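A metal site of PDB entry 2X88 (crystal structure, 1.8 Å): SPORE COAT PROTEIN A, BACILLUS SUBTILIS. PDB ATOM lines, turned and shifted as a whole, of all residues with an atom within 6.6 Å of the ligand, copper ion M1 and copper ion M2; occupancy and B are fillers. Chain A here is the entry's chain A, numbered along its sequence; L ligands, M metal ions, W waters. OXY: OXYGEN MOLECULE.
O of His 491 is in hydrogen-bond range of N of His 422, 2.7 Å away.
NE2 of His 107 lies within hydrogen-bond range of OG1 of Thr 466 (3.1 Å).
A ring nitrogen (NE2) of His 107 lies close to a ring nitrogen (ND1) of His 422 (3.4 Å).
OE1 of Glu 498 sits close to ND1 of His 491 (3.2 Å).
ND1 of His 422 lies within hydrogen-bond range of OG1 of Thr 466 (3.2 Å).
O of His 153 lies within hydrogen-bond range of N of His 105.
O of His 155 lies close to OG1 of Thr 160 (3.4 Å).
O of Val 489 sits at hydrogen-bond distance from N of His 424, 3.1 Å away.
A ring nitrogen (NE2) of His 105 sits close to an oxygen (O2) of the ligand, 3.3 Å away.
A ring nitrogen (NE2) of His 422 lies close to an oxygen (O2) of the ligand (3.5 Å).
Hydrophobic or aromatic side chains within 4 Å of the ligand: His 105, His 107, His 153, His 155, His 422, His 491 and His 493.
Of the 22 residues printed, 8 come within 4 Å of the ligand.
Residues that only touch copper ion M1: His 422 (3.9 Å).
Within 4 Å of copper ion M1: His 155, His 422, His 424 and His 491.
CZ2 of Trp 151 touches copper ion M2 (3.8 Å).
Of the 22 residues printed, 4 come within 4 Å of copper ion M2.
The nearest printed residue that does not touch copper ion M2 is His 105 (4.1 Å).
NE2 of His 424 is bound to copper ion M1, at 2.0 Å.
A ring nitrogen (NE2) of His 491 binds copper ion M1.
Copper ion M1 is bound by a ring nitrogen (NE2) of His 155, at 2.1 Å.
O1 of the ligand is bound to copper ion M1 (2.3 Å).
Copper ion M1 has four donor atoms within binding distance.
Copper ion M2 is bound by a ring nitrogen (ND1) of His 107 (2.0 Å), a ring nitrogen (NE2) of His 153 (2.1 Å), a ring nitrogen (NE2) of His 493 (2.1 Å) and an oxygen (O2) of the ligand (2.5 Å).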
ATOM      1  N   HIS A 105       9.291 -23.534   3.414  1.00  0.00           N
ATOM      2  CA  HIS A 105       9.265 -22.168   2.893  1.00  0.00           C
ATOM      3  C   HIS A 105      10.425 -21.943   1.929  1.00  0.00           C
ATOM      4  O   HIS A 105      11.581 -22.182   2.289  1.00  0.00           O
ATOM      5  CB  HIS A 105       9.314 -21.148   4.039  1.00  0.00           C
ATOM      6  CG  HIS A 105       9.533 -19.734   3.582  1.00  0.00           C
ATOM      7  ND1 HIS A 105       8.684 -19.101   2.699  1.00  0.00           N
ATOM      8  CD2 HIS A 105      10.493 -18.837   3.890  1.00  0.00           C
ATOM      9  CE1 HIS A 105       9.122 -17.866   2.484  1.00  0.00           C
ATOM     10  NE2 HIS A 105      10.212 -17.683   3.192  1.00  0.00           N
ATOM     11  N   LEU A 106      10.107 -21.486   0.726  1.00  0.00           N
ATOM     12  CA  LEU A 106      11.136 -21.054  -0.205  1.00  0.00           C
ATOM     13  C   LEU A 106      11.461 -19.583   0.088  1.00  0.00           C
ATOM     14  O   LEU A 106      10.724 -18.682  -0.309  1.00  0.00           O
ATOM     15  CB  LEU A 106      10.685 -21.244  -1.664  1.00  0.00           C
ATOM     16  CG  LEU A 106      11.689 -20.785  -2.747  1.00  0.00           C
ATOM     17  CD1 LEU A 106      13.042 -21.475  -2.573  1.00  0.00           C
ATOM     18  CD2 LEU A 106      11.129 -21.026  -4.146  1.00  0.00           C
ATOM     19  N   HIS A 107      12.564 -19.380   0.803  1.00  0.00           N
ATOM     20  CA  HIS A 107      13.001 -18.057   1.231  1.00  0.00           C
ATOM     21  C   HIS A 107      13.425 -17.206   0.035  1.00  0.00           C
ATOM     22  O   HIS A 107      14.363 -17.562  -0.691  1.00  0.00           O
ATOM     23  CB  HIS A 107      14.146 -18.161   2.250  1.00  0.00           C
ATOM     24  CG  HIS A 107      14.513 -16.861   2.889  1.00  0.00           C
ATOM     25  ND1 HIS A 107      14.428 -16.644   4.245  1.00  0.00           N
ATOM     26  CD2 HIS A 107      14.974 -15.708   2.349  1.00  0.00           C
ATOM     27  CE1 HIS A 107      14.810 -15.409   4.517  1.00  0.00           C
ATOM     28  NE2 HIS A 107      15.148 -14.822   3.387  1.00  0.00           N
ATOM     29  N   GLY A 108      12.731 -16.093  -0.168  1.00  0.00           N
ATOM     30  CA  GLY A 108      12.944 -15.216  -1.321  1.00  0.00           C
ATOM     31  C   GLY A 108      12.015 -15.507  -2.483  1.00  0.00           C
ATOM     32  O   GLY A 108      12.000 -14.779  -3.475  1.00  0.00           O
ATOM     33  N   GLY A 117       4.557 -21.608   2.420  1.00  0.00           N
ATOM     34  CA  GLY A 117       4.983 -22.284   3.642  1.00  0.00           C
ATOM     35  C   GLY A 117       4.637 -21.499   4.897  1.00  0.00           C
ATOM     36  O   GLY A 117       5.491 -21.303   5.766  1.00  0.00           O
ATOM     37  N   PRO A 119       3.447 -20.640   8.538  1.00  0.00           N
ATOM     38  CA  PRO A 119       3.755 -21.442   9.731  1.00  0.00           C
ATOM     39  C   PRO A 119       2.598 -22.330  10.189  1.00  0.00           C
ATOM     40  O   PRO A 119       2.833 -23.415  10.717  1.00  0.00           O
ATOM     41  CB  PRO A 119       4.074 -20.386  10.797  1.00  0.00           C
ATOM     42  CG  PRO A 119       4.432 -19.162  10.041  1.00  0.00           C
ATOM     43  CD  PRO A 119       3.615 -19.205   8.792  1.00  0.00           C
ATOM     44  N   TRP A 151      16.849 -19.930  -0.825  1.00  0.00           N
ATOM     45  CA  TRP A 151      17.070 -21.153  -0.056  1.00  0.00           C
ATOM     46  C   TRP A 151      15.768 -21.619   0.547  1.00  0.00           C
ATOM     47  O   TRP A 151      14.846 -20.822   0.756  1.00  0.00           O
ATOM     48  CB  TRP A 151      18.198 -20.986   0.983  1.00  0.00           C
ATOM     49  CG  TRP A 151      17.955 -20.041   2.133  1.00  0.00           C
ATOM     50  CD1 TRP A 151      17.735 -18.692   2.074  1.00  0.00           C
ATOM     51  CD2 TRP A 151      17.968 -20.384   3.535  1.00  0.00           C
ATOM     52  NE1 TRP A 151      17.579 -18.179   3.344  1.00  0.00           N
ATOM     53  CE2 TRP A 151      17.723 -19.199   4.257  1.00  0.00           C
ATOM     54  CE3 TRP A 151      18.150 -21.587   4.236  1.00  0.00           C
ATOM     55  CZ2 TRP A 151      17.655 -19.171   5.651  1.00  0.00           C
ATOM     56  CZ3 TRP A 151      18.081 -21.559   5.631  1.00  0.00           C
ATOM     57  CH2 TRP A 151      17.840 -20.358   6.327  1.00  0.00           C
ATOM     58  N   HIS A 153      13.738 -23.998   3.579  1.00  0.00           N
ATOM     59  CA  HIS A 153      13.888 -24.496   4.937  1.00  0.00           C
ATOM     60  C   HIS A 153      12.544 -24.664   5.619  1.00  0.00           C
ATOM     61  O   HIS A 153      11.533 -24.122   5.166  1.00  0.00           O
ATOM     62  CB  HIS A 153      14.807 -23.576   5.774  1.00  0.00           C
ATOM     63  CG  HIS A 153      14.269 -22.185   5.963  1.00  0.00           C
ATOM     64  ND1 HIS A 153      13.310 -21.881   6.909  1.00  0.00           N
ATOM     65  CD2 HIS A 153      14.572 -21.019   5.340  1.00  0.00           C
ATOM     66  CE1 HIS A 153      13.042 -20.587   6.853  1.00  0.00           C
ATOM     67  NE2 HIS A 153      13.794 -20.042   5.914  1.00  0.00           N
ATOM     68  N   ASP A 154      12.528 -25.414   6.719  1.00  0.00           N
ATOM     69  CA  ASP A 154      11.288 -25.617   7.470  1.00  0.00           C
ATOM     70  C   ASP A 154      10.806 -24.325   8.116  1.00  0.00           C
ATOM     71  O   ASP A 154      11.619 -23.474   8.500  1.00  0.00           O
ATOM     72  CB  ASP A 154      11.465 -26.693   8.538  1.00  0.00           C
ATOM     73  CG  ASP A 154      10.143 -27.127   9.122  1.00  0.00           C
ATOM     74  OD1 ASP A 154       9.795 -26.639  10.217  1.00  0.00           O
ATOM     75  OD2 ASP A 154       9.438 -27.911   8.470  1.00  0.00           O
ATOM     76  N   HIS A 155       9.492 -24.186   8.243  1.00  0.00           N
ATOM     77  CA  HIS A 155       8.903 -22.965   8.785  1.00  0.00           C
ATOM     78  C   HIS A 155       7.719 -23.250   9.733  1.00  0.00           C
ATOM     79  O   HIS A 155       6.883 -22.369   9.965  1.00  0.00           O
ATOM     80  CB  HIS A 155       8.448 -22.057   7.624  1.00  0.00           C
ATOM     81  CG  HIS A 155       8.556 -20.595   7.925  1.00  0.00           C
ATOM     82  ND1 HIS A 155       7.938 -20.005   9.018  1.00  0.00           N
ATOM     83  CD2 HIS A 155       9.194 -19.591   7.274  1.00  0.00           C
ATOM     84  CE1 HIS A 155       8.206 -18.710   9.020  1.00  0.00           C
ATOM     85  NE2 HIS A 155       8.961 -18.431   7.971  1.00  0.00           N
ATOM     86  N   THR A 160      10.339 -23.983  14.261  1.00  0.00           N
ATOM     87  CA  THR A 160      11.278 -23.606  13.203  1.00  0.00           C
ATOM     88  C   THR A 160      12.742 -23.704  13.655  1.00  0.00           C
ATOM     89  O   THR A 160      13.583 -24.250  12.927  1.00  0.00           O
ATOM     90  CB  THR A 160      10.925 -22.212  12.613  1.00  0.00           C
ATOM     91  OG1 THR A 160       9.602 -22.276  12.050  1.00  0.00           O
ATOM     92  CG2 THR A 160      11.905 -21.804  11.516  1.00  0.00           C
ATOM     93  N   ALA A 297      19.952 -15.860   7.284  1.00  0.00           N
ATOM     94  CA  ALA A 297      19.106 -15.781   6.083  1.00  0.00           C
ATOM     95  C   ALA A 297      19.578 -14.822   4.988  1.00  0.00           C
ATOM     96  O   ALA A 297      19.053 -14.857   3.875  1.00  0.00           O
ATOM     97  CB  ALA A 297      17.633 -15.511   6.428  1.00  0.00           C
ATOM     98  N   HIS A 422      13.036  -9.942   8.181  1.00  0.00           N
ATOM     99  CA  HIS A 422      12.696 -10.543   6.901  1.00  0.00           C
ATOM    100  C   HIS A 422      11.213 -10.356   6.572  1.00  0.00           C
ATOM    101  O   HIS A 422      10.350 -10.570   7.434  1.00  0.00           O
ATOM    102  CB  HIS A 422      13.073 -12.025   6.916  1.00  0.00           C
ATOM    103  CG  HIS A 422      12.635 -12.777   5.701  1.00  0.00           C
ATOM    104  ND1 HIS A 422      12.958 -12.388   4.421  1.00  0.00           N
ATOM    105  CD2 HIS A 422      11.908 -13.912   5.568  1.00  0.00           C
ATOM    106  CE1 HIS A 422      12.450 -13.230   3.556  1.00  0.00           C
ATOM    107  NE2 HIS A 422      11.800 -14.177   4.222  1.00  0.00           N
ATOM    108  N   HIS A 424       8.334 -11.736   3.811  1.00  0.00           N
ATOM    109  CA  HIS A 424       8.008 -12.704   2.761  1.00  0.00           C
ATOM    110  C   HIS A 424       7.558 -12.027   1.470  1.00  0.00           C
ATOM    111  O   HIS A 424       7.227 -10.831   1.473  1.00  0.00           O
ATOM    112  CB  HIS A 424       6.943 -13.682   3.253  1.00  0.00           C
ATOM    113  CG  HIS A 424       7.457 -14.728   4.191  1.00  0.00           C
ATOM    114  ND1 HIS A 424       6.988 -16.018   4.187  1.00  0.00           N
ATOM    115  CD2 HIS A 424       8.425 -14.671   5.147  1.00  0.00           C
ATOM    116  CE1 HIS A 424       7.624 -16.716   5.118  1.00  0.00           C
ATOM    117  NE2 HIS A 424       8.505 -15.927   5.705  1.00  0.00           N
ATOM    118  N   THR A 466      16.185  -9.749   3.631  1.00  0.00           N
ATOM    119  CA  THR A 466      16.523  -9.886   5.046  1.00  0.00           C
ATOM    120  C   THR A 466      17.550  -8.805   5.377  1.00  0.00           C
ATOM    121  O   THR A 466      18.608  -8.731   4.754  1.00  0.00           O
ATOM    122  CB  THR A 466      17.092 -11.303   5.353  1.00  0.00           C
ATOM    123  OG1 THR A 466      16.161 -12.294   4.901  1.00  0.00           O
ATOM    124  CG2 THR A 466      17.339 -11.483   6.853  1.00  0.00           C
ATOM    125  N   VAL A 489       3.883 -13.391   5.897  1.00  0.00           N
ATOM    126  CA  VAL A 489       4.408 -13.059   7.221  1.00  0.00           C
ATOM    127  C   VAL A 489       5.646 -12.170   7.127  1.00  0.00           C
ATOM    128  O   VAL A 489       6.243 -12.003   6.067  1.00  0.00           O
ATOM    129  CB  VAL A 489       4.763 -14.311   8.101  1.00  0.00           C
ATOM    130  CG1 VAL A 489       3.541 -15.185   8.346  1.00  0.00           C
ATOM    131  CG2 VAL A 489       5.884 -15.120   7.485  1.00  0.00           C
ATOM    132  N   TRP A 490       5.984 -11.551   8.249  1.00  0.00           N
ATOM    133  CA  TRP A 490       7.251 -10.838   8.411  1.00  0.00           C
ATOM    134  C   TRP A 490       7.762 -11.113   9.819  1.00  0.00           C
ATOM    135  O   TRP A 490       6.966 -11.302  10.747  1.00  0.00           O
ATOM    136  CB  TRP A 490       7.124  -9.335   8.104  1.00  0.00           C
ATOM    137  CG  TRP A 490       6.443  -8.509   9.160  1.00  0.00           C
ATOM    138  CD1 TRP A 490       5.108  -8.449   9.429  1.00  0.00           C
ATOM    139  CD2 TRP A 490       7.078  -7.581  10.055  1.00  0.00           C
ATOM    140  NE1 TRP A 490       4.868  -7.563  10.458  1.00  0.00           N
ATOM    141  CE2 TRP A 490       6.059  -7.010  10.853  1.00  0.00           C
ATOM    142  CE3 TRP A 490       8.409  -7.188  10.267  1.00  0.00           C
ATOM    143  CZ2 TRP A 490       6.331  -6.069  11.853  1.00  0.00           C
ATOM    144  CZ3 TRP A 490       8.675  -6.245  11.258  1.00  0.00           C
ATOM    145  CH2 TRP A 490       7.638  -5.694  12.042  1.00  0.00           C
ATOM    146  N   HIS A 491       9.088 -11.179   9.977  1.00  0.00           N
ATOM    147  CA  HIS A 491       9.674 -11.618  11.249  1.00  0.00           C
ATOM    148  C   HIS A 491      11.168 -11.375  11.349  1.00  0.00           C
ATOM    149  O   HIS A 491      11.846 -11.119  10.342  1.00  0.00           O
ATOM    150  CB  HIS A 491       9.389 -13.109  11.484  1.00  0.00           C
ATOM    151  CG  HIS A 491       9.937 -14.017  10.427  1.00  0.00           C
ATOM    152  ND1 HIS A 491      11.169 -14.633  10.537  1.00  0.00           N
ATOM    153  CD2 HIS A 491       9.412 -14.415   9.244  1.00  0.00           C
ATOM    154  CE1 HIS A 491      11.382 -15.369   9.459  1.00  0.00           C
ATOM    155  NE2 HIS A 491      10.334 -15.258   8.669  1.00  0.00           N
ATOM    156  N   HIS A 493      14.681 -13.130  11.711  1.00  0.00           N
ATOM    157  CA  HIS A 493      15.140 -14.436  11.241  1.00  0.00           C
ATOM    158  C   HIS A 493      16.188 -15.083  12.176  1.00  0.00           C
ATOM    159  O   HIS A 493      16.846 -16.064  11.802  1.00  0.00           O
ATOM    160  CB  HIS A 493      15.650 -14.370   9.798  1.00  0.00           C
ATOM    161  CG  HIS A 493      15.388 -15.611   8.991  1.00  0.00           C
ATOM    162  ND1 HIS A 493      16.002 -16.814   9.266  1.00  0.00           N
ATOM    163  CD2 HIS A 493      14.590 -15.828   7.929  1.00  0.00           C
ATOM    164  CE1 HIS A 493      15.583 -17.721   8.403  1.00  0.00           C
ATOM    165  NE2 HIS A 493      14.728 -17.151   7.579  1.00  0.00           N
ATOM    166  N   LEU A 495      16.079 -17.536  14.711  1.00  0.00           N
ATOM    167  CA  LEU A 495      14.997 -18.512  14.843  1.00  0.00           C
ATOM    168  C   LEU A 495      14.486 -18.636  16.267  1.00  0.00           C
ATOM    169  O   LEU A 495      13.298 -18.880  16.479  1.00  0.00           O
ATOM    170  CB  LEU A 495      15.420 -19.873  14.269  1.00  0.00           C
ATOM    171  CG  LEU A 495      15.880 -19.878  12.804  1.00  0.00           C
ATOM    172  CD1 LEU A 495      16.107 -21.305  12.339  1.00  0.00           C
ATOM    173  CD2 LEU A 495      14.885 -19.177  11.873  1.00  0.00           C
ATOM    174  N   GLU A 498      12.125 -15.673  16.435  1.00  0.00           N
ATOM    175  CA  GLU A 498      10.961 -15.959  15.593  1.00  0.00           C
ATOM    176  C   GLU A 498       9.933 -16.842  16.305  1.00  0.00           C
ATOM    177  O   GLU A 498       8.737 -16.569  16.251  1.00  0.00           O
ATOM    178  CB  GLU A 498      11.418 -16.615  14.286  1.00  0.00           C
ATOM    179  CG  GLU A 498      10.301 -17.052  13.342  1.00  0.00           C
ATOM    180  CD  GLU A 498      10.843 -17.688  12.074  1.00  0.00           C
ATOM    181  OE1 GLU A 498      12.019 -17.430  11.724  1.00  0.00           O
ATOM    182  OE2 GLU A 498      10.093 -18.434  11.422  1.00  0.00           O
ATOM    183  N   MET A 503       7.265 -12.658  15.281  1.00  0.00           N
ATOM    184  CA  MET A 503       6.724 -12.961  13.960  1.00  0.00           C
ATOM    185  C   MET A 503       5.268 -12.516  13.905  1.00  0.00           C
ATOM    186  O   MET A 503       4.518 -12.717  14.860  1.00  0.00           O
ATOM    187  CB  MET A 503       6.828 -14.463  13.687  1.00  0.00           C
ATOM    188  CG  MET A 503       6.299 -14.892  12.329  1.00  0.00           C
ATOM    189  SD  MET A 503       6.652 -16.596  11.875  1.00  0.00           S
ATOM    190  CE  MET A 503       5.696 -17.493  13.092  1.00  0.00           C
HETATM  191  O1  OXY L   1      11.708 -17.559   7.164  1.00  0.00           O
HETATM  192  O2  OXY L   1      11.740 -17.123   6.064  1.00  0.00           O
HETATM  193 CU    CU M   1       9.666 -16.582   7.240  1.00  0.00          CU
HETATM  194 CU    CU M   2      14.037 -17.992   5.729  1.00  0.00          CU
HETATM  195 CU    CU M   3      11.039 -15.945   3.750  1.00  0.00          CU
HETATM  196  O   HOH W   1      12.053 -18.685   9.321  1.00  0.00           O
